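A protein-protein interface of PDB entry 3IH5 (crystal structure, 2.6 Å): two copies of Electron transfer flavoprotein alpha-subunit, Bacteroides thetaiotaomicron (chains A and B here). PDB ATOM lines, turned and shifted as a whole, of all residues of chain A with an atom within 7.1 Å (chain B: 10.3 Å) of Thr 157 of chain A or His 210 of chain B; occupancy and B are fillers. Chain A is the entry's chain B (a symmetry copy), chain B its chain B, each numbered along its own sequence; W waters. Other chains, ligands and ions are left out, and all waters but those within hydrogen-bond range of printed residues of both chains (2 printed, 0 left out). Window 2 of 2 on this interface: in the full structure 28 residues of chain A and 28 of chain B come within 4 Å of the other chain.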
ATOM      1  N   SER A 124      28.121 -15.388  -9.826  1.00  0.00           N
ATOM      2  CA  SER A 124      28.291 -16.750 -10.316  1.00  0.00           C
ATOM      3  C   SER A 124      28.403 -16.721 -11.828  1.00  0.00           C
ATOM      4  O   SER A 124      27.820 -15.854 -12.475  1.00  0.00           O
ATOM      5  CB  SER A 124      27.102 -17.627  -9.944  1.00  0.00           C
ATOM      6  OG  SER A 124      27.027 -17.803  -8.548  1.00  0.00           O
ATOM      7  N   GLU A 126      27.990 -19.452 -15.114  1.00  0.00           N
ATOM      8  CA  GLU A 126      27.654 -20.783 -15.597  1.00  0.00           C
ATOM      9  C   GLU A 126      27.612 -20.782 -17.115  1.00  0.00           C
ATOM     10  O   GLU A 126      27.767 -19.739 -17.748  1.00  0.00           O
ATOM     11  CB  GLU A 126      26.307 -21.244 -15.036  1.00  0.00           C
ATOM     12  CG  GLU A 126      26.302 -21.459 -13.537  1.00  0.00           C
ATOM     13  CD  GLU A 126      24.914 -21.758 -12.975  1.00  0.00           C
ATOM     14  OE1 GLU A 126      23.909 -21.617 -13.711  1.00  0.00           O
ATOM     15  OE2 GLU A 126      24.838 -22.127 -11.781  1.00  0.00           O
ATOM     16  N   LEU A 143      27.262 -17.552 -21.932  1.00  0.00           N
ATOM     17  CA  LEU A 143      27.730 -17.309 -20.580  1.00  0.00           C
ATOM     18  C   LEU A 143      26.590 -16.750 -19.723  1.00  0.00           C
ATOM     19  O   LEU A 143      26.055 -15.667 -20.004  1.00  0.00           O
ATOM     20  CB  LEU A 143      28.914 -16.355 -20.588  1.00  0.00           C
ATOM     21  CG  LEU A 143      29.414 -15.994 -19.194  1.00  0.00           C
ATOM     22  CD1 LEU A 143      29.984 -17.232 -18.520  1.00  0.00           C
ATOM     23  CD2 LEU A 143      30.447 -14.886 -19.279  1.00  0.00           C
ATOM     24  N   TYR A 144      26.209 -17.505 -18.695  1.00  0.00           N
ATOM     25  CA  TYR A 144      25.240 -17.049 -17.703  1.00  0.00           C
ATOM     26  C   TYR A 144      25.918 -16.097 -16.723  1.00  0.00           C
ATOM     27  O   TYR A 144      26.796 -16.502 -15.955  1.00  0.00           O
ATOM     28  CB  TYR A 144      24.659 -18.233 -16.921  1.00  0.00           C
ATOM     29  CG  TYR A 144      23.503 -18.963 -17.584  1.00  0.00           C
ATOM     30  CD1 TYR A 144      23.286 -18.880 -18.953  1.00  0.00           C
ATOM     31  CD2 TYR A 144      22.646 -19.763 -16.831  1.00  0.00           C
ATOM     32  CE1 TYR A 144      22.233 -19.550 -19.552  1.00  0.00           C
ATOM     33  CE2 TYR A 144      21.602 -20.447 -17.420  1.00  0.00           C
ATOM     34  CZ  TYR A 144      21.397 -20.337 -18.782  1.00  0.00           C
ATOM     35  OH  TYR A 144      20.354 -21.019 -19.370  1.00  0.00           O
ATOM     36  N   GLN A 145      25.509 -14.833 -16.748  1.00  0.00           N
ATOM     37  CA  GLN A 145      26.077 -13.839 -15.850  1.00  0.00           C
ATOM     38  C   GLN A 145      25.128 -13.604 -14.677  1.00  0.00           C
ATOM     39  O   GLN A 145      24.103 -12.940 -14.806  1.00  0.00           O
ATOM     40  CB  GLN A 145      26.401 -12.561 -16.623  1.00  0.00           C
ATOM     41  CG  GLN A 145      27.369 -12.816 -17.773  1.00  0.00           C
ATOM     42  CD  GLN A 145      27.178 -11.880 -18.948  1.00  0.00           C
ATOM     43  OE1 GLN A 145      27.565 -10.715 -18.902  1.00  0.00           O
ATOM     44  NE2 GLN A 145      26.590 -12.394 -20.019  1.00  0.00           N
ATOM     45  N   ILE A 146      25.482 -14.177 -13.534  1.00  0.00           N
ATOM     46  CA  ILE A 146      24.569 -14.309 -12.407  1.00  0.00           C
ATOM     47  C   ILE A 146      24.898 -13.356 -11.261  1.00  0.00           C
ATOM     48  O   ILE A 146      26.044 -13.274 -10.821  1.00  0.00           O
ATOM     49  CB  ILE A 146      24.581 -15.768 -11.875  1.00  0.00           C
ATOM     50  CG1 ILE A 146      24.266 -16.752 -13.004  1.00  0.00           C
ATOM     51  CG2 ILE A 146      23.606 -15.938 -10.733  1.00  0.00           C
ATOM     52  CD1 ILE A 146      24.622 -18.199 -12.686  1.00  0.00           C
ATOM     53  N   ARG A 147      23.886 -12.644 -10.772  1.00  0.00           N
ATOM     54  CA  ARG A 147      24.059 -11.757  -9.621  1.00  0.00           C
ATOM     55  C   ARG A 147      22.726 -11.301  -9.055  1.00  0.00           C
ATOM     56  O   ARG A 147      21.687 -11.483  -9.688  1.00  0.00           O
ATOM     57  CB  ARG A 147      24.909 -10.529  -9.987  1.00  0.00           C
ATOM     58  CG  ARG A 147      24.517  -9.826 -11.277  1.00  0.00           C
ATOM     59  CD  ARG A 147      25.048  -8.401 -11.312  1.00  0.00           C
ATOM     60  NE  ARG A 147      24.476  -7.603 -10.232  1.00  0.00           N
ATOM     61  CZ  ARG A 147      24.844  -6.362  -9.942  1.00  0.00           C
ATOM     62  NH1 ARG A 147      25.788  -5.769 -10.655  1.00  0.00           N
ATOM     63  NH2 ARG A 147      24.268  -5.714  -8.940  1.00  0.00           N
ATOM     64  N   ALA A 149      19.772  -8.711  -8.154  1.00  0.00           N
ATOM     65  CA  ALA A 149      19.173  -7.783  -9.094  1.00  0.00           C
ATOM     66  C   ALA A 149      17.895  -7.184  -8.521  1.00  0.00           C
ATOM     67  O   ALA A 149      17.379  -7.655  -7.499  1.00  0.00           O
ATOM     68  CB  ALA A 149      18.898  -8.487 -10.402  1.00  0.00           C
ATOM     69  N   ILE A 154      16.047 -10.786  -5.928  1.00  0.00           N
ATOM     70  CA  ILE A 154      16.313 -12.141  -6.376  1.00  0.00           C
ATOM     71  C   ILE A 154      17.685 -12.199  -7.023  1.00  0.00           C
ATOM     72  O   ILE A 154      18.277 -11.160  -7.308  1.00  0.00           O
ATOM     73  CB  ILE A 154      15.319 -12.556  -7.447  1.00  0.00           C
ATOM     74  CG1 ILE A 154      15.477 -11.648  -8.662  1.00  0.00           C
ATOM     75  CG2 ILE A 154      13.906 -12.503  -6.900  1.00  0.00           C
ATOM     76  CD1 ILE A 154      14.620 -12.045  -9.834  1.00  0.00           C
ATOM     77  N   VAL A 155      18.178 -13.415  -7.265  1.00  0.00           N
ATOM     78  CA  VAL A 155      19.406 -13.628  -8.030  1.00  0.00           C
ATOM     79  C   VAL A 155      19.033 -13.938  -9.481  1.00  0.00           C
ATOM     80  O   VAL A 155      18.452 -14.978  -9.768  1.00  0.00           O
ATOM     81  CB  VAL A 155      20.252 -14.803  -7.447  1.00  0.00           C
ATOM     82  CG1 VAL A 155      21.565 -14.972  -8.208  1.00  0.00           C
ATOM     83  CG2 VAL A 155      20.530 -14.590  -5.969  1.00  0.00           C
ATOM     84  N   ALA A 156      19.361 -13.031 -10.397  1.00  0.00           N
ATOM     85  CA  ALA A 156      18.964 -13.183 -11.800  1.00  0.00           C
ATOM     86  C   ALA A 156      20.140 -13.527 -12.690  1.00  0.00           C
ATOM     87  O   ALA A 156      21.297 -13.371 -12.301  1.00  0.00           O
ATOM     88  CB  ALA A 156      18.284 -11.928 -12.311  1.00  0.00           C
ATOM     89  N   THR A 157      19.834 -13.971 -13.900  1.00  0.00           N
ATOM     90  CA  THR A 157      20.863 -14.321 -14.862  1.00  0.00           C
ATOM     91  C   THR A 157      20.753 -13.440 -16.101  1.00  0.00           C
ATOM     92  O   THR A 157      19.666 -13.266 -16.652  1.00  0.00           O
ATOM     93  CB  THR A 157      20.739 -15.789 -15.289  1.00  0.00           C
ATOM     94  OG1 THR A 157      20.787 -16.639 -14.133  1.00  0.00           O
ATOM     95  CG2 THR A 157      21.852 -16.166 -16.257  1.00  0.00           C
ATOM     96  N   ILE A 158      21.878 -12.893 -16.543  1.00  0.00           N
ATOM     97  CA  ILE A 158      21.895 -12.095 -17.758  1.00  0.00           C
ATOM     98  C   ILE A 158      22.623 -12.820 -18.880  1.00  0.00           C
ATOM     99  O   ILE A 158      23.644 -13.473 -18.655  1.00  0.00           O
ATOM    100  CB  ILE A 158      22.515 -10.710 -17.504  1.00  0.00           C
ATOM    101  CG1 ILE A 158      21.449  -9.785 -16.927  1.00  0.00           C
ATOM    102  CG2 ILE A 158      23.040 -10.106 -18.790  1.00  0.00           C
ATOM    103  CD1 ILE A 158      21.842  -9.159 -15.640  1.00  0.00           C
ATOM    104  N   VAL A 159      22.082 -12.719 -20.091  1.00  0.00           N
ATOM    105  CA  VAL A 159      22.738 -13.294 -21.257  1.00  0.00           C
ATOM    106  C   VAL A 159      22.824 -12.303 -22.411  1.00  0.00           C
ATOM    107  O   VAL A 159      21.937 -11.471 -22.605  1.00  0.00           O
ATOM    108  CB  VAL A 159      22.065 -14.617 -21.721  1.00  0.00           C
ATOM    109  CG1 VAL A 159      22.244 -15.699 -20.673  1.00  0.00           C
ATOM    110  CG2 VAL A 159      20.581 -14.401 -22.028  1.00  0.00           C
ATOM    111  N   TYR B 202      20.817  -8.101 -24.743  1.00  0.00           N
ATOM    112  CA  TYR B 202      20.988  -8.600 -23.389  1.00  0.00           C
ATOM    113  C   TYR B 202      19.641  -9.089 -22.956  1.00  0.00           C
ATOM    114  O   TYR B 202      18.630  -8.517 -23.329  1.00  0.00           O
ATOM    115  CB  TYR B 202      21.514  -7.535 -22.424  1.00  0.00           C
ATOM    116  CG  TYR B 202      20.540  -6.430 -22.046  1.00  0.00           C
ATOM    117  CD1 TYR B 202      19.537  -6.641 -21.106  1.00  0.00           C
ATOM    118  CD2 TYR B 202      20.653  -5.162 -22.602  1.00  0.00           C
ATOM    119  CE1 TYR B 202      18.662  -5.629 -20.752  1.00  0.00           C
ATOM    120  CE2 TYR B 202      19.787  -4.149 -22.256  1.00  0.00           C
ATOM    121  CZ  TYR B 202      18.791  -4.383 -21.333  1.00  0.00           C
ATOM    122  OH  TYR B 202      17.930  -3.354 -20.999  1.00  0.00           O
ATOM    123  N   VAL B 203      19.610 -10.170 -22.199  1.00  0.00           N
ATOM    124  CA  VAL B 203      18.338 -10.664 -21.724  1.00  0.00           C
ATOM    125  C   VAL B 203      18.491 -10.972 -20.263  1.00  0.00           C
ATOM    126  O   VAL B 203      19.484 -11.569 -19.842  1.00  0.00           O
ATOM    127  CB  VAL B 203      17.868 -11.905 -22.497  1.00  0.00           C
ATOM    128  CG1 VAL B 203      16.412 -12.187 -22.200  1.00  0.00           C
ATOM    129  CG2 VAL B 203      18.060 -11.701 -23.985  1.00  0.00           C
ATOM    130  N   VAL B 204      17.515 -10.523 -19.490  1.00  0.00           N
ATOM    131  CA  VAL B 204      17.496 -10.765 -18.061  1.00  0.00           C
ATOM    132  C   VAL B 204      16.638 -12.002 -17.822  1.00  0.00           C
ATOM    133  O   VAL B 204      15.487 -12.069 -18.249  1.00  0.00           O
ATOM    134  CB  VAL B 204      16.937  -9.542 -17.311  1.00  0.00           C
ATOM    135  CG1 VAL B 204      17.013  -9.738 -15.800  1.00  0.00           C
ATOM    136  CG2 VAL B 204      17.696  -8.294 -17.726  1.00  0.00           C
ATOM    137  N   LYS B 205      17.213 -12.998 -17.165  1.00  0.00           N
ATOM    138  CA  LYS B 205      16.513 -14.247 -16.917  1.00  0.00           C
ATOM    139  C   LYS B 205      16.525 -14.513 -15.424  1.00  0.00           C
ATOM    140  O   LYS B 205      17.326 -13.935 -14.684  1.00  0.00           O
ATOM    141  CB  LYS B 205      17.195 -15.417 -17.647  1.00  0.00           C
ATOM    142  CG  LYS B 205      17.638 -15.122 -19.081  1.00  0.00           C
ATOM    143  CD  LYS B 205      18.643 -16.164 -19.597  1.00  0.00           C
ATOM    144  CE  LYS B 205      18.070 -17.078 -20.683  1.00  0.00           C
ATOM    145  NZ  LYS B 205      16.755 -17.688 -20.344  1.00  0.00           N
ATOM    146  N   VAL B 206      15.614 -15.363 -14.982  1.00  0.00           N
ATOM    147  CA  VAL B 206      15.774 -16.022 -13.703  1.00  0.00           C
ATOM    148  C   VAL B 206      15.647 -17.524 -13.956  1.00  0.00           C
ATOM    149  O   VAL B 206      14.574 -18.017 -14.316  1.00  0.00           O
ATOM    150  CB  VAL B 206      14.796 -15.510 -12.630  1.00  0.00           C
ATOM    151  CG1 VAL B 206      13.511 -15.003 -13.255  1.00  0.00           C
ATOM    152  CG2 VAL B 206      14.524 -16.593 -11.609  1.00  0.00           C
ATOM    153  N   ILE B 207      16.775 -18.224 -13.814  1.00  0.00           N
ATOM    154  CA  ILE B 207      16.889 -19.653 -14.116  1.00  0.00           C
ATOM    155  C   ILE B 207      16.290 -20.524 -13.013  1.00  0.00           C
ATOM    156  O   ILE B 207      16.555 -20.314 -11.829  1.00  0.00           O
ATOM    157  CB  ILE B 207      18.361 -20.047 -14.358  1.00  0.00           C
ATOM    158  CG1 ILE B 207      18.726 -19.820 -15.819  1.00  0.00           C
ATOM    159  CG2 ILE B 207      18.596 -21.497 -14.015  1.00  0.00           C
ATOM    160  CD1 ILE B 207      19.277 -18.475 -16.093  1.00  0.00           C
ATOM    161  N   GLU B 208      15.471 -21.495 -13.406  1.00  0.00           N
ATOM    162  CA  GLU B 208      14.767 -22.331 -12.435  1.00  0.00           C
ATOM    163  C   GLU B 208      15.722 -23.152 -11.566  1.00  0.00           C
ATOM    164  O   GLU B 208      15.588 -23.178 -10.342  1.00  0.00           O
ATOM    165  CB  GLU B 208      13.753 -23.241 -13.134  1.00  0.00           C
ATOM    166  CG  GLU B 208      12.717 -23.862 -12.199  1.00  0.00           C
ATOM    167  CD  GLU B 208      11.523 -24.456 -12.943  1.00  0.00           C
ATOM    168  OE1 GLU B 208      11.220 -25.656 -12.726  1.00  0.00           O
ATOM    169  OE2 GLU B 208      10.893 -23.718 -13.742  1.00  0.00           O
ATOM    170  N   ARG B 209      16.691 -23.805 -12.198  1.00  0.00           N
ATOM    171  CA  ARG B 209      17.616 -24.679 -11.488  1.00  0.00           C
ATOM    172  C   ARG B 209      18.379 -23.963 -10.355  1.00  0.00           C
ATOM    173  O   ARG B 209      18.965 -24.616  -9.477  1.00  0.00           O
ATOM    174  CB  ARG B 209      18.588 -25.352 -12.472  1.00  0.00           C
ATOM    175  CG  ARG B 209      19.960 -24.726 -12.493  1.00  0.00           C
ATOM    176  CD  ARG B 209      20.800 -25.223 -13.649  1.00  0.00           C
ATOM    177  NE  ARG B 209      21.895 -24.295 -13.912  1.00  0.00           N
ATOM    178  CZ  ARG B 209      22.306 -23.945 -15.128  1.00  0.00           C
ATOM    179  NH1 ARG B 209      23.302 -23.078 -15.269  1.00  0.00           N
ATOM    180  NH2 ARG B 209      21.715 -24.448 -16.213  1.00  0.00           N
ATOM    181  N   HIS B 210      18.359 -22.629 -10.364  1.00  0.00           N
ATOM    182  CA  HIS B 210      19.049 -21.847  -9.333  1.00  0.00           C
ATOM    183  C   HIS B 210      18.293 -21.861  -8.016  1.00  0.00           C
ATOM    184  O   HIS B 210      18.754 -21.326  -7.011  1.00  0.00           O
ATOM    185  CB  HIS B 210      19.248 -20.397  -9.781  1.00  0.00           C
ATOM    186  CG  HIS B 210      20.345 -20.220 -10.783  1.00  0.00           C
ATOM    187  ND1 HIS B 210      20.370 -19.169 -11.671  1.00  0.00           N
ATOM    188  CD2 HIS B 210      21.442 -20.968 -11.042  1.00  0.00           C
ATOM    189  CE1 HIS B 210      21.448 -19.271 -12.431  1.00  0.00           C
ATOM    190  NE2 HIS B 210      22.113 -20.353 -12.076  1.00  0.00           N
ATOM    191  N   VAL B 211      17.126 -22.478  -8.030  1.00  0.00           N
ATOM    192  CA  VAL B 211      16.287 -22.520  -6.850  1.00  0.00           C
ATOM    193  C   VAL B 211      15.967 -23.989  -6.468  1.00  0.00           C
ATOM    194  O   VAL B 211      15.184 -24.272  -5.550  1.00  0.00           O
ATOM    195  CB  VAL B 211      15.030 -21.616  -7.060  1.00  0.00           C
ATOM    196  CG1 VAL B 211      13.823 -22.407  -7.566  1.00  0.00           C
ATOM    197  CG2 VAL B 211      14.710 -20.871  -5.802  1.00  0.00           C
ATOM    198  N   GLU B 212      16.613 -24.918  -7.172  1.00  0.00           N
ATOM    199  CA  GLU B 212      16.490 -26.344  -6.876  1.00  0.00           C
ATOM    200  C   GLU B 212      17.603 -26.783  -5.944  1.00  0.00           C
ATOM    201  O   GLU B 212      18.772 -26.487  -6.188  1.00  0.00           O
ATOM    202  CB  GLU B 212      16.516 -27.173  -8.164  1.00  0.00           C
ATOM    203  CG  GLU B 212      15.192 -27.135  -8.909  1.00  0.00           C
ATOM    204  CD  GLU B 212      15.309 -27.524 -10.372  1.00  0.00           C
ATOM    205  OE1 GLU B 212      16.360 -28.080 -10.761  1.00  0.00           O
ATOM    206  OE2 GLU B 212      14.343 -27.273 -11.135  1.00  0.00           O
ATOM    207  N   LYS B 213      17.239 -27.478  -4.871  1.00  0.00           N
ATOM    208  CA  LYS B 213      18.229 -27.898  -3.881  1.00  0.00           C
ATOM    209  C   LYS B 213      19.431 -28.584  -4.533  1.00  0.00           C
ATOM    210  O   LYS B 213      19.287 -29.425  -5.422  1.00  0.00           O
ATOM    211  CB  LYS B 213      17.616 -28.815  -2.818  1.00  0.00           C
ATOM    212  CG  LYS B 213      17.553 -30.264  -3.250  1.00  0.00           C
ATOM    213  CD  LYS B 213      18.164 -31.196  -2.211  1.00  0.00           C
ATOM    214  CE  LYS B 213      17.243 -31.407  -1.027  1.00  0.00           C
ATOM    215  NZ  LYS B 213      17.860 -32.349  -0.051  1.00  0.00           N
ATOM    216  N   ALA B 214      20.618 -28.204  -4.078  1.00  0.00           N
ATOM    217  CA  ALA B 214      21.856 -28.786  -4.569  1.00  0.00           C
ATOM    218  C   ALA B 214      21.904 -30.280  -4.269  1.00  0.00           C
ATOM    219  O   ALA B 214      21.555 -30.715  -3.168  1.00  0.00           O
ATOM    220  CB  ALA B 214      23.053 -28.082  -3.947  1.00  0.00           C
HETATM  221  O   HOH W   1      18.784 -16.600 -11.933  1.00  0.00           O
HETATM  222  O   HOH W   2      22.737 -24.256 -11.402  1.00  0.00           O
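The backbone NH (N) of Val 203 of chain B is in hydrogen-bond range of the backbone carbonyl oxygen (O) of Val 159 of chain A, at 2.7 Å. O of Thr 157 of chain A sits at hydrogen-bond distance from N of Lys 205 of chain B. The side-chain carboxylate of Glu 126 of chain A lies within salt-bridge range of the guanidinium group of Arg 209 of chain B, at 3.4 Å. A ring nitrogen (NE2) of His 210 of chain B lies within hydrogen-bond range of the side-chain carboxylate (OE1) of Glu 126 of chain A (2.7 Å).
O of Ser 124 of chain A sits at hydrogen-bond distance from N of Ile 146 of chain A (3.1 Å). The backbone carbonyl oxygen (O) of Glu 126 of chain A sits at hydrogen-bond distance from the backbone NH (N) of Tyr 144 of chain A. The backbone carbonyl oxygen (O) of Gln 145 of chain A lies within hydrogen-bond range of the backbone NH (N) of Ile 158 of chain A, 2.8 Å away. The backbone carbonyl oxygen of Arg 147 of chain A is in hydrogen-bond range of the backbone NH of Ala 156 of chain A.
Ile 207 of chain B touches Tyr 144 of chain A. CD2 of Tyr 144 of chain A touches NH1 of Arg 209 of chain B, 3.7 Å away. His 210 of chain B touches Ile 146 of chain A (CE1 to CD1, 3.4 Å). O of Lys 205 of chain B touches CB of Ala 156 of chain A, 3.3 Å away. Thr 157 of chain A touches Val 203 of chain B. Val 204 of chain B touches Thr 157 of chain A. Thr 157 of chain A touches Ile 207 of chain B (OG1 to CD1, 3.1 Å). Thr 157 of chain A touches His 210 of chain B (OG1 to CE1, 3.2 Å). O of Val 159 of chain A touches CA of Tyr 202 of chain B, at 3.1 Å. Lys 205 of chain B touches Val 159 of chain A.
Tyr 144 of chain A touches two residues of chain B. Of chain B, only Val 203, Val 204, Lys 205, Ile 207 and His 210 come within 4 Å of Thr 157 of chain A. Printed residues of chain B within 4 Å of Val 159 of chain A: Tyr 202, Val 203 and Lys 205. Printed residues of chain A within 4 Å of Tyr 202 of chain B: Val 159 (3.1 Å). Val 206 of chain B touches none of the printed residues of chain A. Val 211 of chain B touches none of the printed residues of chain A. The nearest residue of chain A that does not touch His 210 of chain B is Tyr 144 of chain A (4.6 Å). The nearest printed residue of chain A that does not touch Lys 205 of chain B is Ile 158 of chain A (4.7 Å).
Hydrophobic or aromatic side chains of chain B that line the printed part of chain A: Tyr 202, Val 203, Ile 207 and His 210. Of the 14 printed residues of chain A, 7 touch a printed residue of chain B. Among the printed residues, 15 pairs touch across the chains.
No position is printed for both chains.
Water W2 lies within hydrogen-bond range of the guanidinium group (NE) of Arg 209 of chain B (2.6 Å) and the side-chain carboxylate (OE2) of Glu 126 of chain A (3.0 Å). Water W1 lies within hydrogen-bond range of the backbone carbonyl oxygen (O) of Val 155 of chain A (2.7 Å), the side-chain hydroxyl (OG1) of Thr 157 of chain A (3.0 Å), a ring nitrogen (ND1) of His 210 of chain B (3.0 Å) and the backbone NH (N) of Ile 207 of chain B (3.2 Å).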
